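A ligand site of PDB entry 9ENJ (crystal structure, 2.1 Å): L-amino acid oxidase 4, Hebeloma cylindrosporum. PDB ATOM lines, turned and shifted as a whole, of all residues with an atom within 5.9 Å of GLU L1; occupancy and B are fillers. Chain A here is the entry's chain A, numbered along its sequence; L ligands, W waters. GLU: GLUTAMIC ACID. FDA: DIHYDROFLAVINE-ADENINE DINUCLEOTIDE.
Water W2 lies within hydrogen-bond range of O4 of FDA L2 (2.8 Å), OXT of GLU L1 (3.1 Å), NE of Arg 70 (3.4 Å) and SD of Met 69 (3.8 Å).
The side-chain carboxylate (OE2) of Glu 235 is in hydrogen-bond range of the indole nitrogen (NE1) of Trp 506, at 2.8 Å. OH of Tyr 404 lies within hydrogen-bond range of NE1 of Trp 406 (3.2 Å).
The backbone NH (N) of Arg 70 is in hydrogen-bond range of an oxygen (O4) of FDA L2, at 3.2 Å. An oxygen (OXT) of GLU L1 lies within salt-bridge range of the guanidinium group of Arg 70 (2.9 Å). The side-chain carboxylate of Glu 235 sits close to an oxygen (OE2) of GLU L1, 2.5 Å away. An oxygen (OE2) of GLU L1 lies within hydrogen-bond range of the indole nitrogen (NE1) of Trp 506 (3.3 Å). An oxygen (O4) of FDA L2 sits at hydrogen-bond distance from the backbone NH (N) of Met 69 (3.3 Å). A nitrogen (N3) of FDA L2 is in hydrogen-bond range of the backbone carbonyl oxygen of Arg 70 (2.9 Å). The backbone carbonyl oxygen (O) of Ala 505 is in hydrogen-bond range of a nitrogen (N) of GLU L1. O of Trp 506 is in hydrogen-bond range of O3' of FDA L2 (3.1 Å). OXT of GLU L1 lies within hydrogen-bond range of OH of Tyr 404, at 2.7 Å.
Trp 224 touches GLU L1 (CH2 to OE1, 3.8 Å). Phe 239 touches GLU L1. CZ2 of Trp 406 touches CG of GLU L1, at 3.3 Å. Phe 469 touches GLU L1 (CE2 to CB, 3.96 Å). Hydrophobic or aromatic side chains within 4 Å of GLU L1: Trp 224, Phe 239, Tyr 404, Trp 406, Phe 469, Ala 505 and Trp 506. Within 4 Å of GLU L1: Arg 70, Trp 224, Glu 235, Phe 239, Tyr 404, Trp 406, Phe 469, Ala 505 and Trp 506.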
ATOM      1  N   MET A  69       6.554   2.939 -29.064  1.00  0.00           N
ATOM      2  CA  MET A  69       6.160   4.078 -29.878  1.00  0.00           C
ATOM      3  C   MET A  69       4.938   4.819 -29.346  1.00  0.00           C
ATOM      4  O   MET A  69       4.689   5.956 -29.756  1.00  0.00           O
ATOM      5  CB  MET A  69       5.867   3.602 -31.310  1.00  0.00           C
ATOM      6  CG  MET A  69       4.598   2.777 -31.460  1.00  0.00           C
ATOM      7  SD  MET A  69       4.292   2.232 -33.143  1.00  0.00           S
ATOM      8  CE  MET A  69       2.722   1.386 -32.968  1.00  0.00           C
ATOM      9  N   ARG A  70       4.168   4.219 -28.424  1.00  0.00           N
ATOM     10  CA  ARG A  70       2.913   4.813 -27.983  1.00  0.00           C
ATOM     11  C   ARG A  70       2.696   4.562 -26.498  1.00  0.00           C
ATOM     12  O   ARG A  70       2.910   3.448 -26.015  1.00  0.00           O
ATOM     13  CB  ARG A  70       1.721   4.271 -28.787  1.00  0.00           C
ATOM     14  CG  ARG A  70       1.540   2.764 -28.718  1.00  0.00           C
ATOM     15  CD  ARG A  70       0.503   2.310 -29.739  1.00  0.00           C
ATOM     16  NE  ARG A  70       0.354   0.859 -29.790  1.00  0.00           N
ATOM     17  CZ  ARG A  70      -0.316   0.209 -30.732  1.00  0.00           C
ATOM     18  NH1 ARG A  70      -0.917   0.859 -31.728  1.00  0.00           N
ATOM     19  NH2 ARG A  70      -0.395  -1.112 -30.687  1.00  0.00           N
ATOM     20  N   TRP A 224      -3.036 -15.260 -30.408  1.00  0.00           N
ATOM     21  CA  TRP A 224      -3.068 -14.554 -29.136  1.00  0.00           C
ATOM     22  C   TRP A 224      -3.854 -15.326 -28.088  1.00  0.00           C
ATOM     23  O   TRP A 224      -3.442 -15.424 -26.926  1.00  0.00           O
ATOM     24  CB  TRP A 224      -3.668 -13.151 -29.338  1.00  0.00           C
ATOM     25  CG  TRP A 224      -3.764 -12.309 -28.093  1.00  0.00           C
ATOM     26  CD1 TRP A 224      -4.591 -12.518 -27.027  1.00  0.00           C
ATOM     27  CD2 TRP A 224      -3.016 -11.121 -27.799  1.00  0.00           C
ATOM     28  NE1 TRP A 224      -4.403 -11.537 -26.083  1.00  0.00           N
ATOM     29  CE2 TRP A 224      -3.446 -10.665 -26.532  1.00  0.00           C
ATOM     30  CE3 TRP A 224      -2.036 -10.403 -28.480  1.00  0.00           C
ATOM     31  CZ2 TRP A 224      -2.914  -9.529 -25.938  1.00  0.00           C
ATOM     32  CZ3 TRP A 224      -1.511  -9.271 -27.880  1.00  0.00           C
ATOM     33  CH2 TRP A 224      -1.950  -8.844 -26.624  1.00  0.00           C
ATOM     34  N   GLU A 235      -3.651  -6.832 -20.527  1.00  0.00           N
ATOM     35  CA  GLU A 235      -3.468  -5.984 -21.703  1.00  0.00           C
ATOM     36  C   GLU A 235      -4.627  -4.999 -21.846  1.00  0.00           C
ATOM     37  O   GLU A 235      -4.424  -3.858 -22.251  1.00  0.00           O
ATOM     38  CB  GLU A 235      -3.319  -6.851 -22.944  1.00  0.00           C
ATOM     39  CG  GLU A 235      -2.694  -6.104 -24.098  1.00  0.00           C
ATOM     40  CD  GLU A 235      -1.265  -5.688 -23.789  1.00  0.00           C
ATOM     41  OE1 GLU A 235      -0.487  -6.543 -23.306  1.00  0.00           O
ATOM     42  OE2 GLU A 235      -0.949  -4.496 -23.963  1.00  0.00           O
ATOM     43  N   PHE A 239      -4.125  -0.953 -22.095  1.00  0.00           N
ATOM     44  CA  PHE A 239      -4.652  -0.187 -23.209  1.00  0.00           C
ATOM     45  C   PHE A 239      -5.782   0.763 -22.806  1.00  0.00           C
ATOM     46  O   PHE A 239      -6.302   1.480 -23.673  1.00  0.00           O
ATOM     47  CB  PHE A 239      -5.168  -1.132 -24.306  1.00  0.00           C
ATOM     48  CG  PHE A 239      -4.112  -1.562 -25.287  1.00  0.00           C
ATOM     49  CD1 PHE A 239      -3.723  -0.735 -26.324  1.00  0.00           C
ATOM     50  CD2 PHE A 239      -3.519  -2.806 -25.182  1.00  0.00           C
ATOM     51  CE1 PHE A 239      -2.760  -1.130 -27.234  1.00  0.00           C
ATOM     52  CE2 PHE A 239      -2.556  -3.215 -26.082  1.00  0.00           C
ATOM     53  CZ  PHE A 239      -2.177  -2.372 -27.107  1.00  0.00           C
ATOM     54  N   TRP A 249      -3.151   9.264 -25.035  1.00  0.00           N
ATOM     55  CA  TRP A 249      -2.162   8.580 -25.863  1.00  0.00           C
ATOM     56  C   TRP A 249      -1.102   9.582 -26.295  1.00  0.00           C
ATOM     57  O   TRP A 249      -1.415  10.605 -26.909  1.00  0.00           O
ATOM     58  CB  TRP A 249      -2.829   7.922 -27.071  1.00  0.00           C
ATOM     59  CG  TRP A 249      -3.566   6.664 -26.757  1.00  0.00           C
ATOM     60  CD1 TRP A 249      -4.903   6.527 -26.540  1.00  0.00           C
ATOM     61  CD2 TRP A 249      -3.009   5.340 -26.623  1.00  0.00           C
ATOM     62  NE1 TRP A 249      -5.223   5.221 -26.279  1.00  0.00           N
ATOM     63  CE2 TRP A 249      -4.075   4.465 -26.320  1.00  0.00           C
ATOM     64  CE3 TRP A 249      -1.718   4.822 -26.726  1.00  0.00           C
ATOM     65  CZ2 TRP A 249      -3.881   3.101 -26.128  1.00  0.00           C
ATOM     66  CZ3 TRP A 249      -1.526   3.467 -26.531  1.00  0.00           C
ATOM     67  CH2 TRP A 249      -2.608   2.614 -26.238  1.00  0.00           C
ATOM     68  N   TYR A 404       2.942  -4.339 -38.666  1.00  0.00           N
ATOM     69  CA  TYR A 404       3.250  -4.518 -37.249  1.00  0.00           C
ATOM     70  C   TYR A 404       2.466  -5.760 -36.815  1.00  0.00           C
ATOM     71  O   TYR A 404       1.241  -5.724 -36.737  1.00  0.00           O
ATOM     72  CB  TYR A 404       2.862  -3.285 -36.438  1.00  0.00           C
ATOM     73  CG  TYR A 404       3.091  -3.386 -34.941  1.00  0.00           C
ATOM     74  CD1 TYR A 404       4.025  -4.273 -34.409  1.00  0.00           C
ATOM     75  CD2 TYR A 404       2.362  -2.599 -34.060  1.00  0.00           C
ATOM     76  CE1 TYR A 404       4.222  -4.369 -33.041  1.00  0.00           C
ATOM     77  CE2 TYR A 404       2.550  -2.689 -32.684  1.00  0.00           C
ATOM     78  CZ  TYR A 404       3.481  -3.574 -32.189  1.00  0.00           C
ATOM     79  OH  TYR A 404       3.662  -3.663 -30.821  1.00  0.00           O
ATOM     80  N   TRP A 406       2.058  -9.559 -34.421  1.00  0.00           N
ATOM     81  CA  TRP A 406       2.264 -10.301 -33.193  1.00  0.00           C
ATOM     82  C   TRP A 406       2.113 -11.788 -33.460  1.00  0.00           C
ATOM     83  O   TRP A 406       1.693 -12.224 -34.530  1.00  0.00           O
ATOM     84  CB  TRP A 406       1.253  -9.873 -32.118  1.00  0.00           C
ATOM     85  CG  TRP A 406       1.352  -8.453 -31.677  1.00  0.00           C
ATOM     86  CD1 TRP A 406       2.471  -7.678 -31.649  1.00  0.00           C
ATOM     87  CD2 TRP A 406       0.285  -7.641 -31.180  1.00  0.00           C
ATOM     88  NE1 TRP A 406       2.163  -6.426 -31.176  1.00  0.00           N
ATOM     89  CE2 TRP A 406       0.826  -6.377 -30.872  1.00  0.00           C
ATOM     90  CE3 TRP A 406      -1.085  -7.857 -30.964  1.00  0.00           C
ATOM     91  CZ2 TRP A 406       0.059  -5.332 -30.371  1.00  0.00           C
ATOM     92  CZ3 TRP A 406      -1.850  -6.822 -30.466  1.00  0.00           C
ATOM     93  CH2 TRP A 406      -1.277  -5.568 -30.173  1.00  0.00           C
ATOM     94  N   PHE A 469       9.048  -9.619 -26.307  1.00  0.00           N
ATOM     95  CA  PHE A 469       8.756  -9.306 -24.919  1.00  0.00           C
ATOM     96  C   PHE A 469       8.097 -10.509 -24.278  1.00  0.00           C
ATOM     97  O   PHE A 469       7.666 -11.449 -24.960  1.00  0.00           O
ATOM     98  CB  PHE A 469       7.864  -8.064 -24.790  1.00  0.00           C
ATOM     99  CG  PHE A 469       6.893  -7.904 -25.923  1.00  0.00           C
ATOM    100  CD1 PHE A 469       5.900  -8.840 -26.138  1.00  0.00           C
ATOM    101  CD2 PHE A 469       6.968  -6.801 -26.766  1.00  0.00           C
ATOM    102  CE1 PHE A 469       4.998  -8.695 -27.187  1.00  0.00           C
ATOM    103  CE2 PHE A 469       6.078  -6.645 -27.810  1.00  0.00           C
ATOM    104  CZ  PHE A 469       5.093  -7.592 -28.021  1.00  0.00           C
ATOM    105  N   HIS A 504       3.675  -6.515 -19.103  1.00  0.00           N
ATOM    106  CA  HIS A 504       4.541  -7.006 -20.161  1.00  0.00           C
ATOM    107  C   HIS A 504       4.325  -6.197 -21.433  1.00  0.00           C
ATOM    108  O   HIS A 504       3.216  -5.724 -21.712  1.00  0.00           O
ATOM    109  CB  HIS A 504       4.280  -8.480 -20.426  1.00  0.00           C
ATOM    110  CG  HIS A 504       4.687  -9.378 -19.301  1.00  0.00           C
ATOM    111  ND1 HIS A 504       4.098 -10.608 -19.092  1.00  0.00           N
ATOM    112  CD2 HIS A 504       5.613  -9.234 -18.338  1.00  0.00           C
ATOM    113  CE1 HIS A 504       4.650 -11.182 -18.029  1.00  0.00           C
ATOM    114  NE2 HIS A 504       5.580 -10.362 -17.560  1.00  0.00           N
ATOM    115  N   ALA A 505       5.395  -6.023 -22.197  1.00  0.00           N
ATOM    116  CA  ALA A 505       5.349  -5.338 -23.489  1.00  0.00           C
ATOM    117  C   ALA A 505       5.040  -3.855 -23.327  1.00  0.00           C
ATOM    118  O   ALA A 505       4.504  -3.229 -24.249  1.00  0.00           O
ATOM    119  CB  ALA A 505       4.334  -5.999 -24.422  1.00  0.00           C
ATOM    120  N   TRP A 506       5.352  -3.286 -22.168  1.00  0.00           N
ATOM    121  CA  TRP A 506       5.190  -1.856 -21.928  1.00  0.00           C
ATOM    122  C   TRP A 506       6.417  -1.323 -21.207  1.00  0.00           C
ATOM    123  O   TRP A 506       7.075  -2.043 -20.455  1.00  0.00           O
ATOM    124  CB  TRP A 506       3.946  -1.555 -21.077  1.00  0.00           C
ATOM    125  CG  TRP A 506       2.667  -1.911 -21.749  1.00  0.00           C
ATOM    126  CD1 TRP A 506       1.910  -3.026 -21.523  1.00  0.00           C
ATOM    127  CD2 TRP A 506       1.984  -1.162 -22.764  1.00  0.00           C
ATOM    128  NE1 TRP A 506       0.796  -3.010 -22.329  1.00  0.00           N
ATOM    129  CE2 TRP A 506       0.821  -1.876 -23.098  1.00  0.00           C
ATOM    130  CE3 TRP A 506       2.250   0.040 -23.419  1.00  0.00           C
ATOM    131  CZ2 TRP A 506      -0.089  -1.431 -24.059  1.00  0.00           C
ATOM    132  CZ3 TRP A 506       1.347   0.484 -24.372  1.00  0.00           C
ATOM    133  CH2 TRP A 506       0.196  -0.246 -24.681  1.00  0.00           C
HETATM  134  N   GLU L   1       2.395  -2.586 -25.833  1.00  0.00           N
HETATM  135  CA  GLU L   1       2.833  -2.744 -27.222  1.00  0.00           C
HETATM  136  C   GLU L   1       1.890  -2.047 -28.188  1.00  0.00           C
HETATM  137  O   GLU L   1       1.177  -1.109 -27.818  1.00  0.00           O
HETATM  138  CB  GLU L   1       2.946  -4.230 -27.576  1.00  0.00           C
HETATM  139  CG  GLU L   1       1.652  -5.019 -27.528  1.00  0.00           C
HETATM  140  CD  GLU L   1       1.174  -5.290 -26.119  1.00  0.00           C
HETATM  141  OE1 GLU L   1       0.837  -6.452 -25.818  1.00  0.00           O
HETATM  142  OE2 GLU L   1       1.169  -4.341 -25.310  1.00  0.00           O
HETATM  143  OXT GLU L   1       1.826  -2.395 -29.367  1.00  0.00           O
HETATM  144  PA  FDA L   2      15.558  -4.036 -22.962  1.00  0.00           P
HETATM  145  O1A FDA L   2      15.604  -5.284 -23.781  1.00  0.00           O
HETATM  146  O2A FDA L   2      15.002  -2.797 -23.584  1.00  0.00           O
HETATM  147  O5B FDA L   2      17.030  -3.715 -22.404  1.00  0.00           O
HETATM  148  C5B FDA L   2      17.933  -4.805 -22.081  1.00  0.00           C
HETATM  149  C4B FDA L   2      19.353  -4.356 -22.362  1.00  0.00           C
HETATM  150  O4B FDA L   2      20.268  -5.443 -22.074  1.00  0.00           O
HETATM  151  C3B FDA L   2      19.646  -3.943 -23.814  1.00  0.00           C
HETATM  152  O3B FDA L   2      20.416  -2.738 -23.850  1.00  0.00           O
HETATM  153  C2B FDA L   2      20.478  -5.113 -24.352  1.00  0.00           C
HETATM  154  O2B FDA L   2      21.322  -4.762 -25.421  1.00  0.00           O
HETATM  155  C1B FDA L   2      21.233  -5.512 -23.097  1.00  0.00           C
HETATM  156  N9A FDA L   2      21.803  -6.854 -23.095  1.00  0.00           N
HETATM  157  C8A FDA L   2      21.281  -7.983 -23.671  1.00  0.00           C
HETATM  158  N7A FDA L   2      22.032  -9.036 -23.477  1.00  0.00           N
HETATM  159  C5A FDA L   2      23.113  -8.567 -22.739  1.00  0.00           C
HETATM  160  C6A FDA L   2      24.262  -9.208 -22.222  1.00  0.00           C
HETATM  161  N6A FDA L   2      24.515 -10.503 -22.369  1.00  0.00           N
HETATM  162  N1A FDA L   2      25.131  -8.440 -21.528  1.00  0.00           N
HETATM  163  C2A FDA L   2      24.860  -7.128 -21.377  1.00  0.00           C
HETATM  164  N3A FDA L   2      23.823  -6.429 -21.818  1.00  0.00           N
HETATM  165  C4A FDA L   2      22.976  -7.219 -22.495  1.00  0.00           C
HETATM  166  N1  FDA L   2       6.315  -0.255 -24.626  1.00  0.00           N
HETATM  167  C2  FDA L   2       5.526   0.853 -24.489  1.00  0.00           C
HETATM  168  O2  FDA L   2       5.465   1.451 -23.423  1.00  0.00           O
HETATM  169  N3  FDA L   2       4.819   1.261 -25.586  1.00  0.00           N
HETATM  170  C4  FDA L   2       4.836   0.625 -26.819  1.00  0.00           C
HETATM  171  O4  FDA L   2       4.166   1.082 -27.753  1.00  0.00           O
HETATM  172  C4X FDA L   2       5.640  -0.509 -26.934  1.00  0.00           C
HETATM  173  N5  FDA L   2       5.722  -1.205 -28.114  1.00  0.00           N
HETATM  174  C5X FDA L   2       6.677  -2.188 -28.312  1.00  0.00           C
HETATM  175  C6  FDA L   2       6.879  -2.733 -29.564  1.00  0.00           C
HETATM  176  C7  FDA L   2       7.817  -3.695 -29.772  1.00  0.00           C
HETATM  177  C7M FDA L   2       8.011  -4.262 -31.152  1.00  0.00           C
HETATM  178  C8  FDA L   2       8.616  -4.153 -28.668  1.00  0.00           C
HETATM  179  C8M FDA L   2       9.666  -5.220 -28.856  1.00  0.00           C
HETATM  180  C9  FDA L   2       8.409  -3.617 -27.427  1.00  0.00           C
HETATM  181  C9A FDA L   2       7.440  -2.640 -27.217  1.00  0.00           C
HETATM  182  N10 FDA L   2       7.195  -2.069 -25.938  1.00  0.00           N
HETATM  183  C10 FDA L   2       6.399  -0.946 -25.819  1.00  0.00           C
HETATM  184  C1' FDA L   2       7.817  -2.669 -24.728  1.00  0.00           C
HETATM  185  C2' FDA L   2       9.094  -1.956 -24.330  1.00  0.00           C
HETATM  186  O2' FDA L   2       9.845  -1.662 -25.502  1.00  0.00           O
HETATM  187  C3' FDA L   2       9.892  -2.853 -23.386  1.00  0.00           C
HETATM  188  O3' FDA L   2       9.002  -3.417 -22.411  1.00  0.00           O
HETATM  189  C4' FDA L   2      11.021  -2.156 -22.633  1.00  0.00           C
HETATM  190  O4' FDA L   2      11.745  -1.324 -23.538  1.00  0.00           O
HETATM  191  C5' FDA L   2      11.966  -3.166 -22.014  1.00  0.00           C
HETATM  192  O5' FDA L   2      13.059  -2.519 -21.319  1.00  0.00           O
HETATM  193  P   FDA L   2      14.066  -3.423 -20.471  1.00  0.00           P
HETATM  194  O1P FDA L   2      15.113  -2.542 -19.864  1.00  0.00           O
HETATM  195  O2P FDA L   2      13.254  -4.314 -19.594  1.00  0.00           O
HETATM  196  O3P FDA L   2      14.731  -4.329 -21.609  1.00  0.00           O
HETATM  197  O   HOH W   1       1.305  -9.376 -25.930  1.00  0.00           O
HETATM  198  O   HOH W   2       3.637  -0.084 -30.259  1.00  0.00           O
